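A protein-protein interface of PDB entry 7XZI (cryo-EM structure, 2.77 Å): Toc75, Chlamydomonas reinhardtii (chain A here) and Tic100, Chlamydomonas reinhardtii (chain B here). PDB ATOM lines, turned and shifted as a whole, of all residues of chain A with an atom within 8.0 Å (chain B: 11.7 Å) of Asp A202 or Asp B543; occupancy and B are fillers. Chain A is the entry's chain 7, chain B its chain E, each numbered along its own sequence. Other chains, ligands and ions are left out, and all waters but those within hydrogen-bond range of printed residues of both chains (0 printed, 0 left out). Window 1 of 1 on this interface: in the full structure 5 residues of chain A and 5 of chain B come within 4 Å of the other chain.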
ATOM      1  N   LEU A 187     -15.294 -13.882  20.728  1.00  0.00           N
ATOM      2  CA  LEU A 187     -14.466 -12.700  20.916  1.00  0.00           C
ATOM      3  C   LEU A 187     -14.275 -11.961  19.594  1.00  0.00           C
ATOM      4  O   LEU A 187     -14.402 -12.527  18.506  1.00  0.00           O
ATOM      5  CB  LEU A 187     -13.109 -13.082  21.518  1.00  0.00           C
ATOM      6  CG  LEU A 187     -13.118 -13.638  22.944  1.00  0.00           C
ATOM      7  CD1 LEU A 187     -11.714 -14.028  23.384  1.00  0.00           C
ATOM      8  CD2 LEU A 187     -13.720 -12.628  23.908  1.00  0.00           C
ATOM      9  N   THR A 188     -13.952 -10.671  19.706  1.00  0.00           N
ATOM     10  CA  THR A 188     -13.679  -9.862  18.522  1.00  0.00           C
ATOM     11  C   THR A 188     -12.320 -10.208  17.927  1.00  0.00           C
ATOM     12  O   THR A 188     -12.177 -10.329  16.706  1.00  0.00           O
ATOM     13  CB  THR A 188     -13.743  -8.373  18.873  1.00  0.00           C
ATOM     14  OG1 THR A 188     -15.031  -8.063  19.421  1.00  0.00           O
ATOM     15  CG2 THR A 188     -13.505  -7.517  17.640  1.00  0.00           C
ATOM     16  N   GLU A 196      -6.309  -4.113  16.806  1.00  0.00           N
ATOM     17  CA  GLU A 196      -5.831  -2.835  17.315  1.00  0.00           C
ATOM     18  C   GLU A 196      -6.247  -2.699  18.775  1.00  0.00           C
ATOM     19  O   GLU A 196      -6.863  -3.598  19.355  1.00  0.00           O
ATOM     20  CB  GLU A 196      -6.356  -1.669  16.469  1.00  0.00           C
ATOM     21  CG  GLU A 196      -7.868  -1.626  16.329  1.00  0.00           C
ATOM     22  CD  GLU A 196      -8.341  -0.431  15.525  1.00  0.00           C
ATOM     23  OE1 GLU A 196      -7.561   0.531  15.373  1.00  0.00           O
ATOM     24  OE2 GLU A 196      -9.493  -0.457  15.040  1.00  0.00           O
ATOM     25  N   LYS A 197      -5.898  -1.557  19.372  1.00  0.00           N
ATOM     26  CA  LYS A 197      -6.215  -1.328  20.779  1.00  0.00           C
ATOM     27  C   LYS A 197      -7.717  -1.178  20.991  1.00  0.00           C
ATOM     28  O   LYS A 197      -8.242  -1.535  22.053  1.00  0.00           O
ATOM     29  CB  LYS A 197      -5.470  -0.091  21.282  1.00  0.00           C
ATOM     30  CG  LYS A 197      -5.605   0.166  22.773  1.00  0.00           C
ATOM     31  CD  LYS A 197      -4.762   1.356  23.199  1.00  0.00           C
ATOM     32  CE  LYS A 197      -5.182   2.623  22.473  1.00  0.00           C
ATOM     33  NZ  LYS A 197      -4.381   3.800  22.911  1.00  0.00           N
ATOM     34  N   GLN A 198      -8.423  -0.650  19.987  1.00  0.00           N
ATOM     35  CA  GLN A 198      -9.869  -0.493  20.099  1.00  0.00           C
ATOM     36  C   GLN A 198     -10.555  -1.842  20.270  1.00  0.00           C
ATOM     37  O   GLN A 198     -11.514  -1.966  21.044  1.00  0.00           O
ATOM     38  CB  GLN A 198     -10.415   0.234  18.871  1.00  0.00           C
ATOM     39  CG  GLN A 198     -11.917   0.459  18.902  1.00  0.00           C
ATOM     40  CD  GLN A 198     -12.343   1.398  20.011  1.00  0.00           C
ATOM     41  OE1 GLN A 198     -11.580   2.267  20.432  1.00  0.00           O
ATOM     42  NE2 GLN A 198     -13.569   1.228  20.494  1.00  0.00           N
ATOM     43  N   ASP A 199     -10.084  -2.864  19.551  1.00  0.00           N
ATOM     44  CA  ASP A 199     -10.646  -4.201  19.703  1.00  0.00           C
ATOM     45  C   ASP A 199     -10.454  -4.714  21.124  1.00  0.00           C
ATOM     46  O   ASP A 199     -11.369  -5.300  21.713  1.00  0.00           O
ATOM     47  CB  ASP A 199     -10.011  -5.156  18.692  1.00  0.00           C
ATOM     48  CG  ASP A 199     -10.186  -4.690  17.259  1.00  0.00           C
ATOM     49  OD1 ASP A 199     -11.175  -3.981  16.977  1.00  0.00           O
ATOM     50  OD2 ASP A 199      -9.334  -5.033  16.412  1.00  0.00           O
ATOM     51  N   LEU A 200      -9.265  -4.500  21.692  1.00  0.00           N
ATOM     52  CA  LEU A 200      -9.009  -4.935  23.061  1.00  0.00           C
ATOM     53  C   LEU A 200      -9.915  -4.213  24.051  1.00  0.00           C
ATOM     54  O   LEU A 200     -10.473  -4.837  24.961  1.00  0.00           O
ATOM     55  CB  LEU A 200      -7.540  -4.710  23.419  1.00  0.00           C
ATOM     56  CG  LEU A 200      -6.508  -5.393  22.521  1.00  0.00           C
ATOM     57  CD1 LEU A 200      -5.094  -5.083  22.987  1.00  0.00           C
ATOM     58  CD2 LEU A 200      -6.743  -6.893  22.483  1.00  0.00           C
ATOM     59  N   LEU A 201     -10.076  -2.897  23.889  1.00  0.00           N
ATOM     60  CA  LEU A 201     -10.942  -2.148  24.796  1.00  0.00           C
ATOM     61  C   LEU A 201     -12.390  -2.615  24.692  1.00  0.00           C
ATOM     62  O   LEU A 201     -13.064  -2.802  25.713  1.00  0.00           O
ATOM     63  CB  LEU A 201     -10.840  -0.650  24.507  1.00  0.00           C
ATOM     64  CG  LEU A 201      -9.476   0.005  24.736  1.00  0.00           C
ATOM     65  CD1 LEU A 201      -9.498   1.468  24.315  1.00  0.00           C
ATOM     66  CD2 LEU A 201      -9.055  -0.131  26.190  1.00  0.00           C
ATOM     67  N   ASP A 202     -12.882  -2.809  23.465  1.00  0.00           N
ATOM     68  CA  ASP A 202     -14.255  -3.265  23.280  1.00  0.00           C
ATOM     69  C   ASP A 202     -14.457  -4.657  23.865  1.00  0.00           C
ATOM     70  O   ASP A 202     -15.480  -4.924  24.506  1.00  0.00           O
ATOM     71  CB  ASP A 202     -14.623  -3.247  21.796  1.00  0.00           C
ATOM     72  CG  ASP A 202     -14.674  -1.843  21.227  1.00  0.00           C
ATOM     73  OD1 ASP A 202     -14.958  -0.898  21.993  1.00  0.00           O
ATOM     74  OD2 ASP A 202     -14.433  -1.684  20.012  1.00  0.00           O
ATOM     75  N   ASP A 203     -13.495  -5.559  23.652  1.00  0.00           N
ATOM     76  CA  ASP A 203     -13.601  -6.900  24.218  1.00  0.00           C
ATOM     77  C   ASP A 203     -13.609  -6.858  25.738  1.00  0.00           C
ATOM     78  O   ASP A 203     -14.399  -7.560  26.379  1.00  0.00           O
ATOM     79  CB  ASP A 203     -12.458  -7.778  23.713  1.00  0.00           C
ATOM     80  CG  ASP A 203     -12.803  -8.499  22.429  1.00  0.00           C
ATOM     81  OD1 ASP A 203     -13.994  -8.496  22.051  1.00  0.00           O
ATOM     82  OD2 ASP A 203     -11.888  -9.068  21.798  1.00  0.00           O
ATOM     83  N   ARG A 204     -12.737  -6.042  26.337  1.00  0.00           N
ATOM     84  CA  ARG A 204     -12.703  -5.941  27.792  1.00  0.00           C
ATOM     85  C   ARG A 204     -14.025  -5.411  28.334  1.00  0.00           C
ATOM     86  O   ARG A 204     -14.580  -5.960  29.294  1.00  0.00           O
ATOM     87  CB  ARG A 204     -11.546  -5.045  28.230  1.00  0.00           C
ATOM     88  CG  ARG A 204     -11.348  -4.982  29.734  1.00  0.00           C
ATOM     89  CD  ARG A 204     -10.363  -3.890  30.118  1.00  0.00           C
ATOM     90  NE  ARG A 204     -10.879  -2.563  29.812  1.00  0.00           N
ATOM     91  CZ  ARG A 204     -11.653  -1.854  30.627  1.00  0.00           C
ATOM     92  NH1 ARG A 204     -12.025  -2.321  31.807  1.00  0.00           N
ATOM     93  NH2 ARG A 204     -12.063  -0.648  30.246  1.00  0.00           N
ATOM     94  N   ARG A 205     -14.550  -4.347  27.722  1.00  0.00           N
ATOM     95  CA  ARG A 205     -15.812  -3.781  28.188  1.00  0.00           C
ATOM     96  C   ARG A 205     -16.955  -4.779  28.037  1.00  0.00           C
ATOM     97  O   ARG A 205     -17.773  -4.941  28.950  1.00  0.00           O
ATOM     98  CB  ARG A 205     -16.121  -2.491  27.429  1.00  0.00           C
ATOM     99  CG  ARG A 205     -17.461  -1.871  27.782  1.00  0.00           C
ATOM    100  CD  ARG A 205     -17.515  -1.453  29.241  1.00  0.00           C
ATOM    101  NE  ARG A 205     -16.755  -0.237  29.492  1.00  0.00           N
ATOM    102  CZ  ARG A 205     -16.624   0.333  30.686  1.00  0.00           C
ATOM    103  NH1 ARG A 205     -17.181  -0.192  31.766  1.00  0.00           N
ATOM    104  NH2 ARG A 205     -15.919   1.454  30.796  1.00  0.00           N
ATOM    105  N   LYS A 206     -17.017  -5.468  26.895  1.00  0.00           N
ATOM    106  CA  LYS A 206     -18.088  -6.431  26.656  1.00  0.00           C
ATOM    107  C   LYS A 206     -18.011  -7.596  27.634  1.00  0.00           C
ATOM    108  O   LYS A 206     -19.033  -8.040  28.171  1.00  0.00           O
ATOM    109  CB  LYS A 206     -18.022  -6.924  25.211  1.00  0.00           C
ATOM    110  CG  LYS A 206     -19.052  -7.984  24.860  1.00  0.00           C
ATOM    111  CD  LYS A 206     -18.984  -8.346  23.383  1.00  0.00           C
ATOM    112  CE  LYS A 206     -17.586  -8.793  22.984  1.00  0.00           C
ATOM    113  NZ  LYS A 206     -17.478  -9.047  21.521  1.00  0.00           N
ATOM    114  N   LEU A 207     -16.803  -8.112  27.876  1.00  0.00           N
ATOM    115  CA  LEU A 207     -16.645  -9.222  28.810  1.00  0.00           C
ATOM    116  C   LEU A 207     -16.988  -8.799  30.233  1.00  0.00           C
ATOM    117  O   LEU A 207     -17.584  -9.574  30.988  1.00  0.00           O
ATOM    118  CB  LEU A 207     -15.222  -9.775  28.735  1.00  0.00           C
ATOM    119  CG  LEU A 207     -14.880 -10.537  27.453  1.00  0.00           C
ATOM    120  CD1 LEU A 207     -13.451 -11.055  27.489  1.00  0.00           C
ATOM    121  CD2 LEU A 207     -15.862 -11.676  27.235  1.00  0.00           C
ATOM    122  N   GLU A 208     -16.610  -7.579  30.624  1.00  0.00           N
ATOM    123  CA  GLU A 208     -16.985  -7.088  31.945  1.00  0.00           C
ATOM    124  C   GLU A 208     -18.496  -6.956  32.078  1.00  0.00           C
ATOM    125  O   GLU A 208     -19.069  -7.315  33.113  1.00  0.00           O
ATOM    126  CB  GLU A 208     -16.307  -5.746  32.228  1.00  0.00           C
ATOM    127  CG  GLU A 208     -14.873  -5.862  32.714  1.00  0.00           C
ATOM    128  CD  GLU A 208     -14.281  -4.527  33.120  1.00  0.00           C
ATOM    129  OE1 GLU A 208     -14.946  -3.491  32.910  1.00  0.00           O
ATOM    130  OE2 GLU A 208     -13.150  -4.513  33.650  1.00  0.00           O
ATOM    131  N   ILE A 209     -19.160  -6.438  31.044  1.00  0.00           N
ATOM    132  CA  ILE A 209     -20.598  -6.202  31.136  1.00  0.00           C
ATOM    133  C   ILE A 209     -21.378  -7.513  31.133  1.00  0.00           C
ATOM    134  O   ILE A 209     -22.298  -7.698  31.937  1.00  0.00           O
ATOM    135  CB  ILE A 209     -21.054  -5.265  30.003  1.00  0.00           C
ATOM    136  CG1 ILE A 209     -20.502  -3.857  30.226  1.00  0.00           C
ATOM    137  CG2 ILE A 209     -22.570  -5.227  29.918  1.00  0.00           C
ATOM    138  CD1 ILE A 209     -20.918  -3.243  31.542  1.00  0.00           C
ATOM    139  N   ILE A 220      -6.474  -7.763  29.702  1.00  0.00           N
ATOM    140  CA  ILE A 220      -6.015  -8.218  28.396  1.00  0.00           C
ATOM    141  C   ILE A 220      -4.619  -7.658  28.176  1.00  0.00           C
ATOM    142  O   ILE A 220      -4.409  -6.442  28.273  1.00  0.00           O
ATOM    143  CB  ILE A 220      -6.970  -7.780  27.276  1.00  0.00           C
ATOM    144  CG1 ILE A 220      -8.412  -8.142  27.635  1.00  0.00           C
ATOM    145  CG2 ILE A 220      -6.575  -8.426  25.962  1.00  0.00           C
ATOM    146  CD1 ILE A 220      -9.434  -7.622  26.649  1.00  0.00           C
ATOM    147  N   GLU B 532     -11.209   3.197  36.679  1.00  0.00           N
ATOM    148  CA  GLU B 532     -10.628   2.389  35.604  1.00  0.00           C
ATOM    149  C   GLU B 532     -11.104   2.847  34.229  1.00  0.00           C
ATOM    150  O   GLU B 532     -11.422   2.030  33.362  1.00  0.00           O
ATOM    151  CB  GLU B 532     -10.934   0.903  35.811  1.00  0.00           C
ATOM    152  N   GLY B 533     -11.168   4.164  34.025  1.00  0.00           N
ATOM    153  CA  GLY B 533     -11.694   4.705  32.784  1.00  0.00           C
ATOM    154  C   GLY B 533     -10.900   4.326  31.552  1.00  0.00           C
ATOM    155  O   GLY B 533     -11.466   4.279  30.455  1.00  0.00           O
ATOM    156  N   ALA B 534      -9.612   4.048  31.709  1.00  0.00           N
ATOM    157  CA  ALA B 534      -8.699   3.733  30.605  1.00  0.00           C
ATOM    158  C   ALA B 534      -8.846   4.814  29.534  1.00  0.00           C
ATOM    159  O   ALA B 534      -9.144   5.970  29.849  1.00  0.00           O
ATOM    160  CB  ALA B 534      -8.954   2.316  30.120  1.00  0.00           C
ATOM    161  N   THR B 535      -8.650   4.449  28.265  1.00  0.00           N
ATOM    162  CA  THR B 535      -8.853   5.353  27.133  1.00  0.00           C
ATOM    163  C   THR B 535      -8.061   6.651  27.327  1.00  0.00           C
ATOM    164  O   THR B 535      -8.620   7.732  27.525  1.00  0.00           O
ATOM    165  CB  THR B 535     -10.343   5.645  26.924  1.00  0.00           C
ATOM    166  OG1 THR B 535     -10.845   6.407  28.031  1.00  0.00           O
ATOM    167  CG2 THR B 535     -11.126   4.348  26.815  1.00  0.00           C
ATOM    168  N   SER B 537      -6.677   8.693  25.504  1.00  0.00           N
ATOM    169  CA  SER B 537      -7.391   9.730  24.775  1.00  0.00           C
ATOM    170  C   SER B 537      -8.712   9.155  24.288  1.00  0.00           C
ATOM    171  O   SER B 537      -8.746   8.063  23.712  1.00  0.00           O
ATOM    172  CB  SER B 537      -6.567  10.254  23.595  1.00  0.00           C
ATOM    173  OG  SER B 537      -6.155   9.191  22.754  1.00  0.00           O
ATOM    174  N   GLU B 538      -9.800   9.886  24.515  1.00  0.00           N
ATOM    175  CA  GLU B 538     -11.120   9.381  24.155  1.00  0.00           C
ATOM    176  C   GLU B 538     -11.429   9.533  22.674  1.00  0.00           C
ATOM    177  O   GLU B 538     -12.599   9.439  22.288  1.00  0.00           O
ATOM    178  CB  GLU B 538     -12.206  10.063  24.990  1.00  0.00           C
ATOM    179  CG  GLU B 538     -12.462   9.369  26.318  1.00  0.00           C
ATOM    180  CD  GLU B 538     -13.812   9.713  26.915  1.00  0.00           C
ATOM    181  OE1 GLU B 538     -14.413  10.721  26.488  1.00  0.00           O
ATOM    182  OE2 GLU B 538     -14.275   8.970  27.806  1.00  0.00           O
ATOM    183  N   GLU B 539     -10.413   9.769  21.842  1.00  0.00           N
ATOM    184  CA  GLU B 539     -10.593   9.643  20.402  1.00  0.00           C
ATOM    185  C   GLU B 539     -10.820   8.193  19.995  1.00  0.00           C
ATOM    186  O   GLU B 539     -11.218   7.934  18.855  1.00  0.00           O
ATOM    187  CB  GLU B 539      -9.384  10.231  19.671  1.00  0.00           C
ATOM    188  CG  GLU B 539      -8.039   9.691  20.126  1.00  0.00           C
ATOM    189  CD  GLU B 539      -7.622   8.459  19.356  1.00  0.00           C
ATOM    190  OE1 GLU B 539      -8.239   8.182  18.308  1.00  0.00           O
ATOM    191  OE2 GLU B 539      -6.682   7.765  19.796  1.00  0.00           O
ATOM    192  N   ASN B 540     -10.562   7.248  20.902  1.00  0.00           N
ATOM    193  CA  ASN B 540     -10.989   5.862  20.773  1.00  0.00           C
ATOM    194  C   ASN B 540     -12.277   5.679  21.568  1.00  0.00           C
ATOM    195  O   ASN B 540     -12.226   5.375  22.767  1.00  0.00           O
ATOM    196  CB  ASN B 540      -9.906   4.905  21.277  1.00  0.00           C
ATOM    197  CG  ASN B 540      -8.712   4.824  20.347  1.00  0.00           C
ATOM    198  OD1 ASN B 540      -8.589   5.605  19.404  1.00  0.00           O
ATOM    199  ND2 ASN B 540      -7.822   3.875  20.608  1.00  0.00           N
ATOM    200  N   PRO B 541     -13.438   5.853  20.949  1.00  0.00           N
ATOM    201  CA  PRO B 541     -14.698   5.822  21.692  1.00  0.00           C
ATOM    202  C   PRO B 541     -15.191   4.395  21.910  1.00  0.00           C
ATOM    203  O   PRO B 541     -14.694   3.435  21.320  1.00  0.00           O
ATOM    204  CB  PRO B 541     -15.665   6.601  20.781  1.00  0.00           C
ATOM    205  CG  PRO B 541     -14.891   6.901  19.499  1.00  0.00           C
ATOM    206  CD  PRO B 541     -13.666   6.049  19.512  1.00  0.00           C
ATOM    207  N   MET B 542     -16.191   4.279  22.778  1.00  0.00           N
ATOM    208  CA  MET B 542     -16.821   2.999  23.058  1.00  0.00           C
ATOM    209  C   MET B 542     -17.810   2.649  21.954  1.00  0.00           C
ATOM    210  O   MET B 542     -18.354   3.528  21.282  1.00  0.00           O
ATOM    211  CB  MET B 542     -17.531   3.029  24.412  1.00  0.00           C
ATOM    212  CG  MET B 542     -18.602   4.097  24.521  1.00  0.00           C
ATOM    213  SD  MET B 542     -19.163   4.327  26.216  1.00  0.00           S
ATOM    214  CE  MET B 542     -19.669   2.661  26.630  1.00  0.00           C
ATOM    215  N   ASP B 543     -18.028   1.352  21.768  1.00  0.00           N
ATOM    216  CA  ASP B 543     -18.913   0.887  20.705  1.00  0.00           C
ATOM    217  C   ASP B 543     -20.338   1.364  20.968  1.00  0.00           C
ATOM    218  O   ASP B 543     -20.806   1.303  22.111  1.00  0.00           O
ATOM    219  CB  ASP B 543     -18.870  -0.636  20.606  1.00  0.00           C
ATOM    220  CG  ASP B 543     -19.362  -1.146  19.265  1.00  0.00           C
ATOM    221  OD1 ASP B 543     -18.723  -0.831  18.239  1.00  0.00           O
ATOM    222  OD2 ASP B 543     -20.382  -1.865  19.237  1.00  0.00           O
ATOM    223  N   PRO B 544     -21.048   1.858  19.950  1.00  0.00           N
ATOM    224  CA  PRO B 544     -22.402   2.392  20.185  1.00  0.00           C
ATOM    225  C   PRO B 544     -23.381   1.381  20.759  1.00  0.00           C
ATOM    226  O   PRO B 544     -24.239   1.760  21.568  1.00  0.00           O
ATOM    227  CB  PRO B 544     -22.834   2.862  18.789  1.00  0.00           C
ATOM    228  CG  PRO B 544     -21.554   3.108  18.059  1.00  0.00           C
ATOM    229  CD  PRO B 544     -20.603   2.066  18.562  1.00  0.00           C
ATOM    230  N   ARG B 545     -23.289   0.109  20.360  1.00  0.00           N
ATOM    231  CA  ARG B 545     -24.215  -0.896  20.877  1.00  0.00           C
ATOM    232  C   ARG B 545     -24.080  -1.043  22.386  1.00  0.00           C
ATOM    233  O   ARG B 545     -25.082  -1.041  23.116  1.00  0.00           O
ATOM    234  CB  ARG B 545     -23.962  -2.239  20.191  1.00  0.00           C
ATOM    235  CG  ARG B 545     -23.689  -2.141  18.700  1.00  0.00           C
ATOM    236  CD  ARG B 545     -23.001  -3.397  18.180  1.00  0.00           C
ATOM    237  NE  ARG B 545     -23.837  -4.583  18.304  1.00  0.00           N
ATOM    238  CZ  ARG B 545     -23.463  -5.806  17.944  1.00  0.00           C
ATOM    239  NH1 ARG B 545     -22.262  -6.042  17.440  1.00  0.00           N
ATOM    240  NH2 ARG B 545     -24.315  -6.815  18.094  1.00  0.00           N
ATOM    241  N   ILE B 546     -22.841  -1.166  22.869  1.00  0.00           N
ATOM    242  CA  ILE B 546     -22.595  -1.264  24.304  1.00  0.00           C
ATOM    243  C   ILE B 546     -23.085  -0.007  25.008  1.00  0.00           C
ATOM    244  O   ILE B 546     -23.673  -0.074  26.093  1.00  0.00           O
ATOM    245  CB  ILE B 546     -21.100  -1.513  24.570  1.00  0.00           C
ATOM    246  CG1 ILE B 546     -20.595  -2.694  23.739  1.00  0.00           C
ATOM    247  CG2 ILE B 546     -20.854  -1.757  26.047  1.00  0.00           C
ATOM    248  CD1 ILE B 546     -21.249  -4.011  24.087  1.00  0.00           C
ATOM    249  N   ARG B 547     -22.854   1.155  24.397  1.00  0.00           N
ATOM    250  CA  ARG B 547     -23.273   2.417  24.995  1.00  0.00           C
ATOM    251  C   ARG B 547     -24.784   2.462  25.190  1.00  0.00           C
ATOM    252  O   ARG B 547     -25.274   2.813  26.270  1.00  0.00           O
ATOM    253  CB  ARG B 547     -22.801   3.574  24.117  1.00  0.00           C
ATOM    254  CG  ARG B 547     -23.188   4.952  24.606  1.00  0.00           C
ATOM    255  CD  ARG B 547     -22.717   6.007  23.621  1.00  0.00           C
ATOM    256  NE  ARG B 547     -23.228   5.755  22.281  1.00  0.00           N
ATOM    257  CZ  ARG B 547     -22.864   6.434  21.198  1.00  0.00           C
ATOM    258  NH1 ARG B 547     -21.978   7.414  21.261  1.00  0.00           N
ATOM    259  NH2 ARG B 547     -23.403   6.120  20.025  1.00  0.00           N
ATOM    260  N   GLU B 548     -25.542   2.089  24.157  1.00  0.00           N
ATOM    261  CA  GLU B 548     -27.000   2.118  24.258  1.00  0.00           C
ATOM    262  C   GLU B 548     -27.513   1.077  25.246  1.00  0.00           C
ATOM    263  O   GLU B 548     -28.453   1.342  26.010  1.00  0.00           O
ATOM    264  CB  GLU B 548     -27.624   1.905  22.880  1.00  0.00           C
ATOM    265  CG  GLU B 548     -27.224   2.953  21.856  1.00  0.00           C
ATOM    266  CD  GLU B 548     -27.756   4.331  22.195  1.00  0.00           C
ATOM    267  OE1 GLU B 548     -28.792   4.418  22.885  1.00  0.00           O
ATOM    268  OE2 GLU B 548     -27.135   5.330  21.773  1.00  0.00           O
ATOM    269  N   LEU B 549     -26.916  -0.117  25.241  1.00  0.00           N
ATOM    270  CA  LEU B 549     -27.329  -1.152  26.184  1.00  0.00           C
ATOM    271  C   LEU B 549     -27.111  -0.693  27.622  1.00  0.00           C
ATOM    272  O   LEU B 549     -27.983  -0.863  28.485  1.00  0.00           O
ATOM    273  CB  LEU B 549     -26.565  -2.445  25.900  1.00  0.00           C
ATOM    274  CG  LEU B 549     -26.888  -3.668  26.760  1.00  0.00           C
ATOM    275  CD1 LEU B 549     -28.324  -4.113  26.536  1.00  0.00           C
ATOM    276  CD2 LEU B 549     -25.917  -4.803  26.469  1.00  0.00           C
ATOM    277  N   MET B 550     -25.955  -0.084  27.889  1.00  0.00           N
ATOM    278  CA  MET B 550     -25.667   0.401  29.234  1.00  0.00           C
ATOM    279  C   MET B 550     -26.555   1.584  29.599  1.00  0.00           C
ATOM    280  O   MET B 550     -26.909   1.756  30.767  1.00  0.00           O
ATOM    281  CB  MET B 550     -24.188   0.769  29.352  1.00  0.00           C
ATOM    282  CG  MET B 550     -23.251  -0.408  29.136  1.00  0.00           C
ATOM    283  SD  MET B 550     -21.511   0.059  29.110  1.00  0.00           S
ATOM    284  CE  MET B 550     -21.236   0.397  30.842  1.00  0.00           C
ATOM    285  N   ALA B 551     -26.930   2.409  28.618  1.00  0.00           N
ATOM    286  CA  ALA B 551     -27.865   3.496  28.899  1.00  0.00           C
ATOM    287  C   ALA B 551     -29.227   2.957  29.324  1.00  0.00           C
ATOM    288  O   ALA B 551     -29.829   3.449  30.288  1.00  0.00           O
ATOM    289  CB  ALA B 551     -28.003   4.401  27.676  1.00  0.00           C
ATOM    290  N   ALA B 552     -29.724   1.936  28.622  1.00  0.00           N
ATOM    291  CA  ALA B 552     -30.995   1.326  29.010  1.00  0.00           C
ATOM    292  C   ALA B 552     -30.901   0.680  30.389  1.00  0.00           C
ATOM    293  O   ALA B 552     -31.829   0.786  31.208  1.00  0.00           O
ATOM    294  CB  ALA B 552     -31.426   0.302  27.961  1.00  0.00           C
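The backbone carbonyl oxygen of Pro B541 sits at hydrogen-bond distance from the side-chain amide nitrogen of Gln A198, 2.6 Å away.
OD1 of Asn B540 lies close to OE1 of Glu B539 (2.8 Å).
OD1 of Asp A202 lies within hydrogen-bond range of NE2 of Gln A198 (2.9 Å).
Among the printed residues, pairs that only touch across the chains: Gln A198 with Asn B540, Lys A197 with Asn B540, Ile A209 with Met B550, Arg A205 with Ile B546 and Asp A202 with Asp B543.
Gln A198 touches just these residues of chain B: Asn B540 (3.2 Å) and Pro B541 (2.6 Å).
No residue of chain B comes within 4 Å of Leu A201.
Asp A202 touches just one residue of chain B: Asp B543.
No residue of chain B comes within 4 Å of Asp A203.
Printed residues of chain B within 4 Å of Ile A209: Met B550 (3.7 Å).
Glu B538 touches none of the printed residues of chain A.
Of the printed residues of chain A, Asn B540 touches Lys A197 and Gln A198.
Of the printed residues of chain A, Pro B541 touches Gln A198.
Asp B543 touches just one residue of chain A: Asp A202 (3.8 Å).
No residue of chain A comes within 4 Å of Pro B544.
Of the printed residues of chain A, Ile B546 touches Arg A205 (3.8 Å).
Printed residues of chain A within 4 Å of Met B550: Ile A209.
Ala B552 touches none of the printed residues of chain A.
The nearest residue of chain A that does not touch Asp B543 is Gln A198 (4.6 Å).
The nearest printed residue of chain B that does not touch Ile A209 is Ile B546 (4.7 Å).
Printed residues of chain B that touch a printed residue of chain A: Asn B540, Pro B541, Asp B543, Ile B546 and Met B550.
Hydrophobic or aromatic side chains of chain B that line the printed part of chain A: Ile B546 and Met B550.
Of the 17 printed residues of chain A, 5 touch a printed residue of chain B.
Printed residues of chain A that touch a printed residue of chain B: Lys A197, Gln A198, Asp A202, Arg A205 and Ile A209.
Hydrophobic or aromatic side chains of chain A within 4 Å of the printed part of chain B: Ile A209.
Among the printed residues, 6 pairs touch across the chains.
Among the printed residues, no Asp or Glu carboxylate lies within 4 Å of a Lys or Arg side-chain nitrogen of the other chain.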
